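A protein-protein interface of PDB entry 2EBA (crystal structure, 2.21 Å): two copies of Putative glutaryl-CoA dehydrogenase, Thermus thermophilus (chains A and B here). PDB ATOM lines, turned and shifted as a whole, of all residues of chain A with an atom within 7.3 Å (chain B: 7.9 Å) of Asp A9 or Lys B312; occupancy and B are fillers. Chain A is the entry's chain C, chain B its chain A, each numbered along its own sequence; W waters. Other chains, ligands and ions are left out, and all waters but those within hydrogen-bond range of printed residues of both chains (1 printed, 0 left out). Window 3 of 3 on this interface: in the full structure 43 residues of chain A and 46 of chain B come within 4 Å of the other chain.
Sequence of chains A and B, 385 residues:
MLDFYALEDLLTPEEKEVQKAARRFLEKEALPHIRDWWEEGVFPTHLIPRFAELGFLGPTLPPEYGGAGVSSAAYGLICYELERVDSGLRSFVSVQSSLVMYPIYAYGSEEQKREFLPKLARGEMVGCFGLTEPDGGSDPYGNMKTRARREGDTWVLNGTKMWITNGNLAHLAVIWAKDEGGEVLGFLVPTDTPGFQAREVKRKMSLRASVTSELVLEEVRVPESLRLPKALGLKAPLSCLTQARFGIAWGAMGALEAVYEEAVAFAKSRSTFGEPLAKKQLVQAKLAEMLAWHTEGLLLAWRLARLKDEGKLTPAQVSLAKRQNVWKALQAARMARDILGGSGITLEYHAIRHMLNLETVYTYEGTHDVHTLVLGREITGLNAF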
ATOM      1  N   ASP A   3      18.246   1.115  20.231  1.00  0.00           N
ATOM      2  CA  ASP A   3      19.132   2.277  20.345  1.00  0.00           C
ATOM      3  C   ASP A   3      19.198   3.037  19.025  1.00  0.00           C
ATOM      4  O   ASP A   3      20.174   2.911  18.266  1.00  0.00           O
ATOM      5  CB  ASP A   3      20.525   1.758  20.767  1.00  0.00           C
ATOM      6  CG  ASP A   3      21.539   2.852  20.987  1.00  0.00           C
ATOM      7  OD1 ASP A   3      21.147   4.001  21.237  1.00  0.00           O
ATOM      8  OD2 ASP A   3      22.746   2.544  20.924  1.00  0.00           O
ATOM      9  N   TYR A   5      19.684   6.278  18.558  1.00  0.00           N
ATOM     10  CA  TYR A   5      20.728   7.318  18.444  1.00  0.00           C
ATOM     11  C   TYR A   5      22.125   6.775  18.729  1.00  0.00           C
ATOM     12  O   TYR A   5      23.034   7.535  19.038  1.00  0.00           O
ATOM     13  CB  TYR A   5      20.456   8.490  19.382  1.00  0.00           C
ATOM     14  CG  TYR A   5      19.725   9.622  18.721  1.00  0.00           C
ATOM     15  CD1 TYR A   5      18.915   9.394  17.604  1.00  0.00           C
ATOM     16  CD2 TYR A   5      19.764  10.907  19.257  1.00  0.00           C
ATOM     17  CE1 TYR A   5      18.153  10.420  17.040  1.00  0.00           C
ATOM     18  CE2 TYR A   5      18.999  11.945  18.702  1.00  0.00           C
ATOM     19  CZ  TYR A   5      18.196  11.688  17.599  1.00  0.00           C
ATOM     20  OH  TYR A   5      17.404  12.681  17.074  1.00  0.00           O
ATOM     21  N   ALA A   6      22.272   5.454  18.649  1.00  0.00           N
ATOM     22  CA  ALA A   6      23.547   4.765  18.878  1.00  0.00           C
ATOM     23  C   ALA A   6      24.291   5.208  20.131  1.00  0.00           C
ATOM     24  O   ALA A   6      25.472   5.547  20.067  1.00  0.00           O
ATOM     25  CB  ALA A   6      24.439   4.932  17.664  1.00  0.00           C
ATOM     26  N   LEU A   7      23.603   5.195  21.267  1.00  0.00           N
ATOM     27  CA  LEU A   7      24.220   5.607  22.517  1.00  0.00           C
ATOM     28  C   LEU A   7      25.190   4.537  23.018  1.00  0.00           C
ATOM     29  O   LEU A   7      26.078   4.817  23.824  1.00  0.00           O
ATOM     30  CB  LEU A   7      23.137   5.936  23.559  1.00  0.00           C
ATOM     31  CG  LEU A   7      22.518   7.350  23.446  1.00  0.00           C
ATOM     32  CD1 LEU A   7      23.475   8.372  24.036  1.00  0.00           C
ATOM     33  CD2 LEU A   7      22.216   7.718  21.986  1.00  0.00           C
ATOM     34  N   GLU A   8      25.036   3.321  22.504  1.00  0.00           N
ATOM     35  CA  GLU A   8      25.910   2.230  22.893  1.00  0.00           C
ATOM     36  C   GLU A   8      27.339   2.606  22.542  1.00  0.00           C
ATOM     37  O   GLU A   8      28.298   2.023  23.048  1.00  0.00           O
ATOM     38  CB  GLU A   8      25.503   0.942  22.183  1.00  0.00           C
ATOM     39  CG  GLU A   8      24.340   0.229  22.854  1.00  0.00           C
ATOM     40  CD  GLU A   8      23.808  -0.914  22.022  1.00  0.00           C
ATOM     41  OE1 GLU A   8      23.503  -0.669  20.833  1.00  0.00           O
ATOM     42  OE2 GLU A   8      23.691  -2.044  22.551  1.00  0.00           O
ATOM     43  N   ASP A   9      27.464   3.599  21.669  1.00  0.00           N
ATOM     44  CA  ASP A   9      28.756   4.108  21.246  1.00  0.00           C
ATOM     45  C   ASP A   9      29.388   4.908  22.371  1.00  0.00           C
ATOM     46  O   ASP A   9      30.593   5.121  22.391  1.00  0.00           O
ATOM     47  CB  ASP A   9      28.593   5.037  20.046  1.00  0.00           C
ATOM     48  CG  ASP A   9      28.501   4.293  18.732  1.00  0.00           C
ATOM     49  OD1 ASP A   9      28.545   3.050  18.751  1.00  0.00           O
ATOM     50  OD2 ASP A   9      28.391   4.963  17.679  1.00  0.00           O
ATOM     51  N   LEU A  10      28.562   5.377  23.291  1.00  0.00           N
ATOM     52  CA  LEU A  10      29.054   6.170  24.395  1.00  0.00           C
ATOM     53  C   LEU A  10      29.367   5.315  25.613  1.00  0.00           C
ATOM     54  O   LEU A  10      29.699   5.840  26.683  1.00  0.00           O
ATOM     55  CB  LEU A  10      28.013   7.226  24.746  1.00  0.00           C
ATOM     56  CG  LEU A  10      27.532   8.087  23.574  1.00  0.00           C
ATOM     57  CD1 LEU A  10      26.456   9.030  24.060  1.00  0.00           C
ATOM     58  CD2 LEU A  10      28.689   8.879  23.002  1.00  0.00           C
ATOM     59  N   LEU A  11      29.276   3.997  25.437  1.00  0.00           N
ATOM     60  CA  LEU A  11      29.515   3.054  26.518  1.00  0.00           C
ATOM     61  C   LEU A  11      30.862   2.350  26.461  1.00  0.00           C
ATOM     62  O   LEU A  11      31.377   2.042  25.385  1.00  0.00           O
ATOM     63  CB  LEU A  11      28.395   2.020  26.535  1.00  0.00           C
ATOM     64  CG  LEU A  11      26.992   2.599  26.698  1.00  0.00           C
ATOM     65  CD1 LEU A  11      25.978   1.499  26.536  1.00  0.00           C
ATOM     66  CD2 LEU A  11      26.850   3.251  28.059  1.00  0.00           C
ATOM     67  N   THR A  12      31.431   2.100  27.636  1.00  0.00           N
ATOM     68  CA  THR A  12      32.707   1.410  27.721  1.00  0.00           C
ATOM     69  C   THR A  12      32.427  -0.053  27.394  1.00  0.00           C
ATOM     70  O   THR A  12      31.281  -0.478  27.336  1.00  0.00           O
ATOM     71  CB  THR A  12      33.308   1.509  29.145  1.00  0.00           C
ATOM     72  OG1 THR A  12      32.471   0.812  30.075  1.00  0.00           O
ATOM     73  CG2 THR A  12      33.429   2.954  29.576  1.00  0.00           C
ATOM     74  N   LYS A  16      29.126  -2.377  28.356  1.00  0.00           N
ATOM     75  CA  LYS A  16      28.389  -3.036  27.293  1.00  0.00           C
ATOM     76  C   LYS A  16      28.305  -4.527  27.522  1.00  0.00           C
ATOM     77  O   LYS A  16      27.394  -5.178  27.024  1.00  0.00           O
ATOM     78  CB  LYS A  16      29.023  -2.766  25.936  1.00  0.00           C
ATOM     79  CG  LYS A  16      28.714  -1.384  25.419  1.00  0.00           C
ATOM     80  CD  LYS A  16      29.170  -1.179  23.979  1.00  0.00           C
ATOM     81  CE  LYS A  16      30.674  -1.077  23.869  1.00  0.00           C
ATOM     82  NZ  LYS A  16      31.036  -0.260  22.681  1.00  0.00           N
ATOM     83  N   TRP A 302      21.692   8.327  30.297  1.00  0.00           N
ATOM     84  CA  TRP A 302      23.122   8.264  30.014  1.00  0.00           C
ATOM     85  C   TRP A 302      23.856   9.466  30.609  1.00  0.00           C
ATOM     86  O   TRP A 302      24.876   9.314  31.283  1.00  0.00           O
ATOM     87  CB  TRP A 302      23.361   8.226  28.507  1.00  0.00           C
ATOM     88  CG  TRP A 302      24.765   8.588  28.134  1.00  0.00           C
ATOM     89  CD1 TRP A 302      25.864   7.777  28.171  1.00  0.00           C
ATOM     90  CD2 TRP A 302      25.242   9.893  27.786  1.00  0.00           C
ATOM     91  NE1 TRP A 302      26.996   8.498  27.876  1.00  0.00           N
ATOM     92  CE2 TRP A 302      26.643   9.800  27.638  1.00  0.00           C
ATOM     93  CE3 TRP A 302      24.619  11.131  27.590  1.00  0.00           C
ATOM     94  CZ2 TRP A 302      27.435  10.905  27.305  1.00  0.00           C
ATOM     95  CZ3 TRP A 302      25.406  12.231  27.257  1.00  0.00           C
ATOM     96  CH2 TRP A 302      26.799  12.109  27.119  1.00  0.00           C
ATOM     97  N   ARG A 306      26.820   9.701  33.807  1.00  0.00           N
ATOM     98  CA  ARG A 306      28.135  10.312  33.786  1.00  0.00           C
ATOM     99  C   ARG A 306      28.257  11.391  34.861  1.00  0.00           C
ATOM    100  O   ARG A 306      29.264  11.467  35.564  1.00  0.00           O
ATOM    101  CB  ARG A 306      28.425  10.903  32.397  1.00  0.00           C
ATOM    102  CG  ARG A 306      28.438   9.889  31.226  1.00  0.00           C
ATOM    103  CD  ARG A 306      29.357   8.678  31.497  1.00  0.00           C
ATOM    104  NE  ARG A 306      29.440   7.739  30.373  1.00  0.00           N
ATOM    105  CZ  ARG A 306      29.725   6.439  30.490  1.00  0.00           C
ATOM    106  NH1 ARG A 306      29.962   5.900  31.680  1.00  0.00           N
ATOM    107  NH2 ARG A 306      29.764   5.672  29.410  1.00  0.00           N
ATOM    108  N   ARG B 303      23.717  14.929  20.271  1.00  0.00           N
ATOM    109  CA  ARG B 303      23.986  13.578  19.775  1.00  0.00           C
ATOM    110  C   ARG B 303      24.077  13.518  18.261  1.00  0.00           C
ATOM    111  O   ARG B 303      24.932  12.842  17.699  1.00  0.00           O
ATOM    112  CB  ARG B 303      22.888  12.616  20.251  1.00  0.00           C
ATOM    113  CG  ARG B 303      23.040  11.184  19.749  1.00  0.00           C
ATOM    114  CD  ARG B 303      24.431  10.731  20.027  1.00  0.00           C
ATOM    115  NE  ARG B 303      24.723   9.394  19.548  1.00  0.00           N
ATOM    116  CZ  ARG B 303      25.952   8.992  19.265  1.00  0.00           C
ATOM    117  NH1 ARG B 303      26.958   9.842  19.411  1.00  0.00           N
ATOM    118  NH2 ARG B 303      26.177   7.751  18.860  1.00  0.00           N
ATOM    119  N   LEU B 304      23.169  14.232  17.615  1.00  0.00           N
ATOM    120  CA  LEU B 304      23.090  14.289  16.174  1.00  0.00           C
ATOM    121  C   LEU B 304      24.289  15.026  15.596  1.00  0.00           C
ATOM    122  O   LEU B 304      24.744  14.706  14.512  1.00  0.00           O
ATOM    123  CB  LEU B 304      21.796  15.004  15.779  1.00  0.00           C
ATOM    124  CG  LEU B 304      20.863  14.266  14.819  1.00  0.00           C
ATOM    125  CD1 LEU B 304      20.512  12.894  15.376  1.00  0.00           C
ATOM    126  CD2 LEU B 304      19.623  15.090  14.590  1.00  0.00           C
ATOM    127  N   ARG B 306      27.350  15.075  16.806  1.00  0.00           N
ATOM    128  CA  ARG B 306      28.504  14.189  16.814  1.00  0.00           C
ATOM    129  C   ARG B 306      28.363  13.136  15.723  1.00  0.00           C
ATOM    130  O   ARG B 306      29.297  12.910  14.963  1.00  0.00           O
ATOM    131  CB  ARG B 306      28.676  13.529  18.189  1.00  0.00           C
ATOM    132  CG  ARG B 306      28.917  14.527  19.329  1.00  0.00           C
ATOM    133  CD  ARG B 306      30.096  15.475  19.065  1.00  0.00           C
ATOM    134  NE  ARG B 306      30.366  16.353  20.206  1.00  0.00           N
ATOM    135  CZ  ARG B 306      30.950  17.549  20.125  1.00  0.00           C
ATOM    136  NH1 ARG B 306      31.335  18.030  18.951  1.00  0.00           N
ATOM    137  NH2 ARG B 306      31.139  18.277  21.217  1.00  0.00           N
ATOM    138  N   LEU B 307      27.199  12.504  15.636  1.00  0.00           N
ATOM    139  CA  LEU B 307      26.981  11.504  14.598  1.00  0.00           C
ATOM    140  C   LEU B 307      27.257  12.124  13.225  1.00  0.00           C
ATOM    141  O   LEU B 307      27.837  11.492  12.344  1.00  0.00           O
ATOM    142  CB  LEU B 307      25.539  10.982  14.644  1.00  0.00           C
ATOM    143  CG  LEU B 307      25.149   9.987  15.734  1.00  0.00           C
ATOM    144  CD1 LEU B 307      23.638   9.781  15.721  1.00  0.00           C
ATOM    145  CD2 LEU B 307      25.875   8.674  15.506  1.00  0.00           C
ATOM    146  N   LYS B 308      26.846  13.377  13.058  1.00  0.00           N
ATOM    147  CA  LYS B 308      27.015  14.061  11.792  1.00  0.00           C
ATOM    148  C   LYS B 308      28.475  14.196  11.369  1.00  0.00           C
ATOM    149  O   LYS B 308      28.823  13.899  10.228  1.00  0.00           O
ATOM    150  CB  LYS B 308      26.357  15.431  11.853  1.00  0.00           C
ATOM    151  CG  LYS B 308      26.240  16.065  10.497  1.00  0.00           C
ATOM    152  CD  LYS B 308      25.635  17.449  10.552  1.00  0.00           C
ATOM    153  CE  LYS B 308      25.668  18.080   9.171  1.00  0.00           C
ATOM    154  NZ  LYS B 308      25.240  19.498   9.185  1.00  0.00           N
ATOM    155  N   ASP B 309      29.330  14.631  12.284  1.00  0.00           N
ATOM    156  CA  ASP B 309      30.730  14.785  11.958  1.00  0.00           C
ATOM    157  C   ASP B 309      31.457  13.466  11.776  1.00  0.00           C
ATOM    158  O   ASP B 309      32.479  13.423  11.098  1.00  0.00           O
ATOM    159  CB  ASP B 309      31.444  15.624  13.011  1.00  0.00           C
ATOM    160  CG  ASP B 309      31.066  17.086  12.931  1.00  0.00           C
ATOM    161  OD1 ASP B 309      30.866  17.559  11.799  1.00  0.00           O
ATOM    162  OD2 ASP B 309      30.970  17.765  13.979  1.00  0.00           O
ATOM    163  N   GLU B 310      30.947  12.390  12.367  1.00  0.00           N
ATOM    164  CA  GLU B 310      31.598  11.091  12.211  1.00  0.00           C
ATOM    165  C   GLU B 310      31.005  10.305  11.035  1.00  0.00           C
ATOM    166  O   GLU B 310      31.306   9.126  10.829  1.00  0.00           O
ATOM    167  CB  GLU B 310      31.543  10.287  13.528  1.00  0.00           C
ATOM    168  CG  GLU B 310      30.173  10.026  14.127  1.00  0.00           C
ATOM    169  CD  GLU B 310      30.221   9.811  15.643  1.00  0.00           C
ATOM    170  OE1 GLU B 310      29.431   8.985  16.144  1.00  0.00           O
ATOM    171  OE2 GLU B 310      31.025  10.476  16.333  1.00  0.00           O
ATOM    172  N   GLY B 311      30.175  10.998  10.257  1.00  0.00           N
ATOM    173  CA  GLY B 311      29.555  10.413   9.081  1.00  0.00           C
ATOM    174  C   GLY B 311      28.540   9.325   9.323  1.00  0.00           C
ATOM    175  O   GLY B 311      28.306   8.506   8.434  1.00  0.00           O
ATOM    176  N   LYS B 312      27.902   9.314  10.489  1.00  0.00           N
ATOM    177  CA  LYS B 312      26.911   8.286  10.802  1.00  0.00           C
ATOM    178  C   LYS B 312      25.501   8.805  10.964  1.00  0.00           C
ATOM    179  O   LYS B 312      24.618   8.078  11.449  1.00  0.00           O
ATOM    180  CB  LYS B 312      27.290   7.569  12.081  1.00  0.00           C
ATOM    181  CG  LYS B 312      28.644   7.010  11.970  1.00  0.00           C
ATOM    182  CD  LYS B 312      28.840   5.953  13.008  1.00  0.00           C
ATOM    183  CE  LYS B 312      29.798   6.453  14.056  1.00  0.00           C
ATOM    184  NZ  LYS B 312      30.350   5.281  14.786  1.00  0.00           N
ATOM    185  N   LEU B 313      25.283  10.059  10.599  1.00  0.00           N
ATOM    186  CA  LEU B 313      23.958  10.632  10.741  1.00  0.00           C
ATOM    187  C   LEU B 313      23.034  10.207   9.603  1.00  0.00           C
ATOM    188  O   LEU B 313      23.415  10.300   8.446  1.00  0.00           O
ATOM    189  CB  LEU B 313      24.074  12.144  10.783  1.00  0.00           C
ATOM    190  CG  LEU B 313      22.749  12.870  10.936  1.00  0.00           C
ATOM    191  CD1 LEU B 313      22.051  12.425  12.218  1.00  0.00           C
ATOM    192  CD2 LEU B 313      23.002  14.353  10.940  1.00  0.00           C
ATOM    193  N   THR B 314      21.829   9.733   9.923  1.00  0.00           N
ATOM    194  CA  THR B 314      20.885   9.335   8.885  1.00  0.00           C
ATOM    195  C   THR B 314      19.740  10.332   8.851  1.00  0.00           C
ATOM    196  O   THR B 314      19.502  11.048   9.813  1.00  0.00           O
ATOM    197  CB  THR B 314      20.290   7.933   9.115  1.00  0.00           C
ATOM    198  OG1 THR B 314      19.249   8.012  10.095  1.00  0.00           O
ATOM    199  CG2 THR B 314      21.374   6.950   9.567  1.00  0.00           C
ATOM    200  N   PRO B 315      19.014  10.399   7.733  1.00  0.00           N
ATOM    201  CA  PRO B 315      17.898  11.349   7.634  1.00  0.00           C
ATOM    202  C   PRO B 315      16.788  11.096   8.651  1.00  0.00           C
ATOM    203  O   PRO B 315      16.209  12.036   9.195  1.00  0.00           O
ATOM    204  CB  PRO B 315      17.409  11.159   6.208  1.00  0.00           C
ATOM    205  CG  PRO B 315      18.649  10.714   5.488  1.00  0.00           C
ATOM    206  CD  PRO B 315      19.267   9.746   6.440  1.00  0.00           C
ATOM    207  N   GLN B 317      17.050   9.954  11.574  1.00  0.00           N
ATOM    208  CA  GLN B 317      17.487  10.463  12.871  1.00  0.00           C
ATOM    209  C   GLN B 317      17.238  11.969  12.930  1.00  0.00           C
ATOM    210  O   GLN B 317      16.762  12.489  13.936  1.00  0.00           O
ATOM    211  CB  GLN B 317      18.982  10.174  13.095  1.00  0.00           C
ATOM    212  CG  GLN B 317      19.335   8.702  13.137  1.00  0.00           C
ATOM    213  CD  GLN B 317      20.813   8.452  13.406  1.00  0.00           C
ATOM    214  OE1 GLN B 317      21.687   8.988  12.716  1.00  0.00           O
ATOM    215  NE2 GLN B 317      21.098   7.622  14.408  1.00  0.00           N
HETATM  216  O   HOH W   1      29.416   7.878  18.468  1.00  0.00           O
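The backbone carbonyl oxygen (O) of Gln B317 is in hydrogen-bond range of the side-chain hydroxyl (OH) of Tyr A5 (3.2 Å).
OD2 of Asp A9 lies within salt-bridge range of NH2 of Arg B303 (3.8 Å).
The guanidinium group (NH2) of Arg B303 lies within hydrogen-bond range of the backbone carbonyl oxygen (O) of Ala A6 (2.6 Å).
NZ of Lys B312 lies within salt-bridge range of OD2 of Asp A9, 3.5 Å away.
The guanidinium group of Arg B303 lies within hydrogen-bond range of the backbone carbonyl oxygen of Tyr A5 (2.6 Å).
1 position is printed for both chains.
Of the 12 printed residues of chain A, 4 touch a printed residue of chain B.
Printed residues of chain A that touch a printed residue of chain B: Tyr A5, Ala A6, Leu A7 and Asp A9.
Of the 13 printed residues of chain B, 4 touch a printed residue of chain A.
Hydrophobic or aromatic side chains of chain B within 4 Å of the printed part of chain A: Leu B304.
Among the printed residues, Asp or Glu carboxylates within 4 Å of a Lys or Arg side-chain nitrogen of the other chain: Asp A9 with Arg B303 (3.8 Å) and Asp A9 with Lys B312 (3.5 Å).
The side-chain carboxylate (OD1) of Asp A3 lies within hydrogen-bond range of the backbone NH (N) of Leu A7, at 2.7 Å.
N of Ala A6 sits at hydrogen-bond distance from OD1 of Asp A3 (3.2 Å).
The backbone NH (N) of Thr B314 is in hydrogen-bond range of the side-chain amide oxygen (OE1) of Gln B317 (2.9 Å).
O of Lys B312 lies close to OE1 of Gln B317, at 3.3 Å.
N of Lys B312 sits at hydrogen-bond distance from O of Leu B307 (2.9 Å).
Water W1 lies within hydrogen-bond range of the side-chain carboxylate of Glu B310, the side-chain carboxylate of Asp A9 and the guanidinium group of Arg B303.
Leu B304 touches Tyr A5 (CD1 to CZ, 3.4 Å).
NE of Arg B303 touches CD2 of Leu A7, at 3.9 Å.
Of the printed residues of chain B, Tyr A5 touches Arg B303, Leu B304 and Gln B317.
Of the printed residues of chain B, Ala A6 touches Arg B303 (2.6 Å).
Printed residues of chain B within 4 Å of Leu A7: Arg B303 (3.9 Å).
Leu A11 touches none of the printed residues of chain B.
Of the printed residues of chain A, Arg B303 touches Tyr A5 (2.6 Å), Ala A6 (2.6 Å), Leu A7 (3.9 Å) and Asp A9 (3.8 Å).
Asp B309 touches none of the printed residues of chain A.
Of chain A, only Asp A9 comes within 4 Å of Lys B312.
Of the printed residues of chain A, Gln B317 touches Tyr A5 (3.2 Å).
The nearest printed residue of chain A that does not touch Gln B317 is Ala A6 (4.9 Å).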
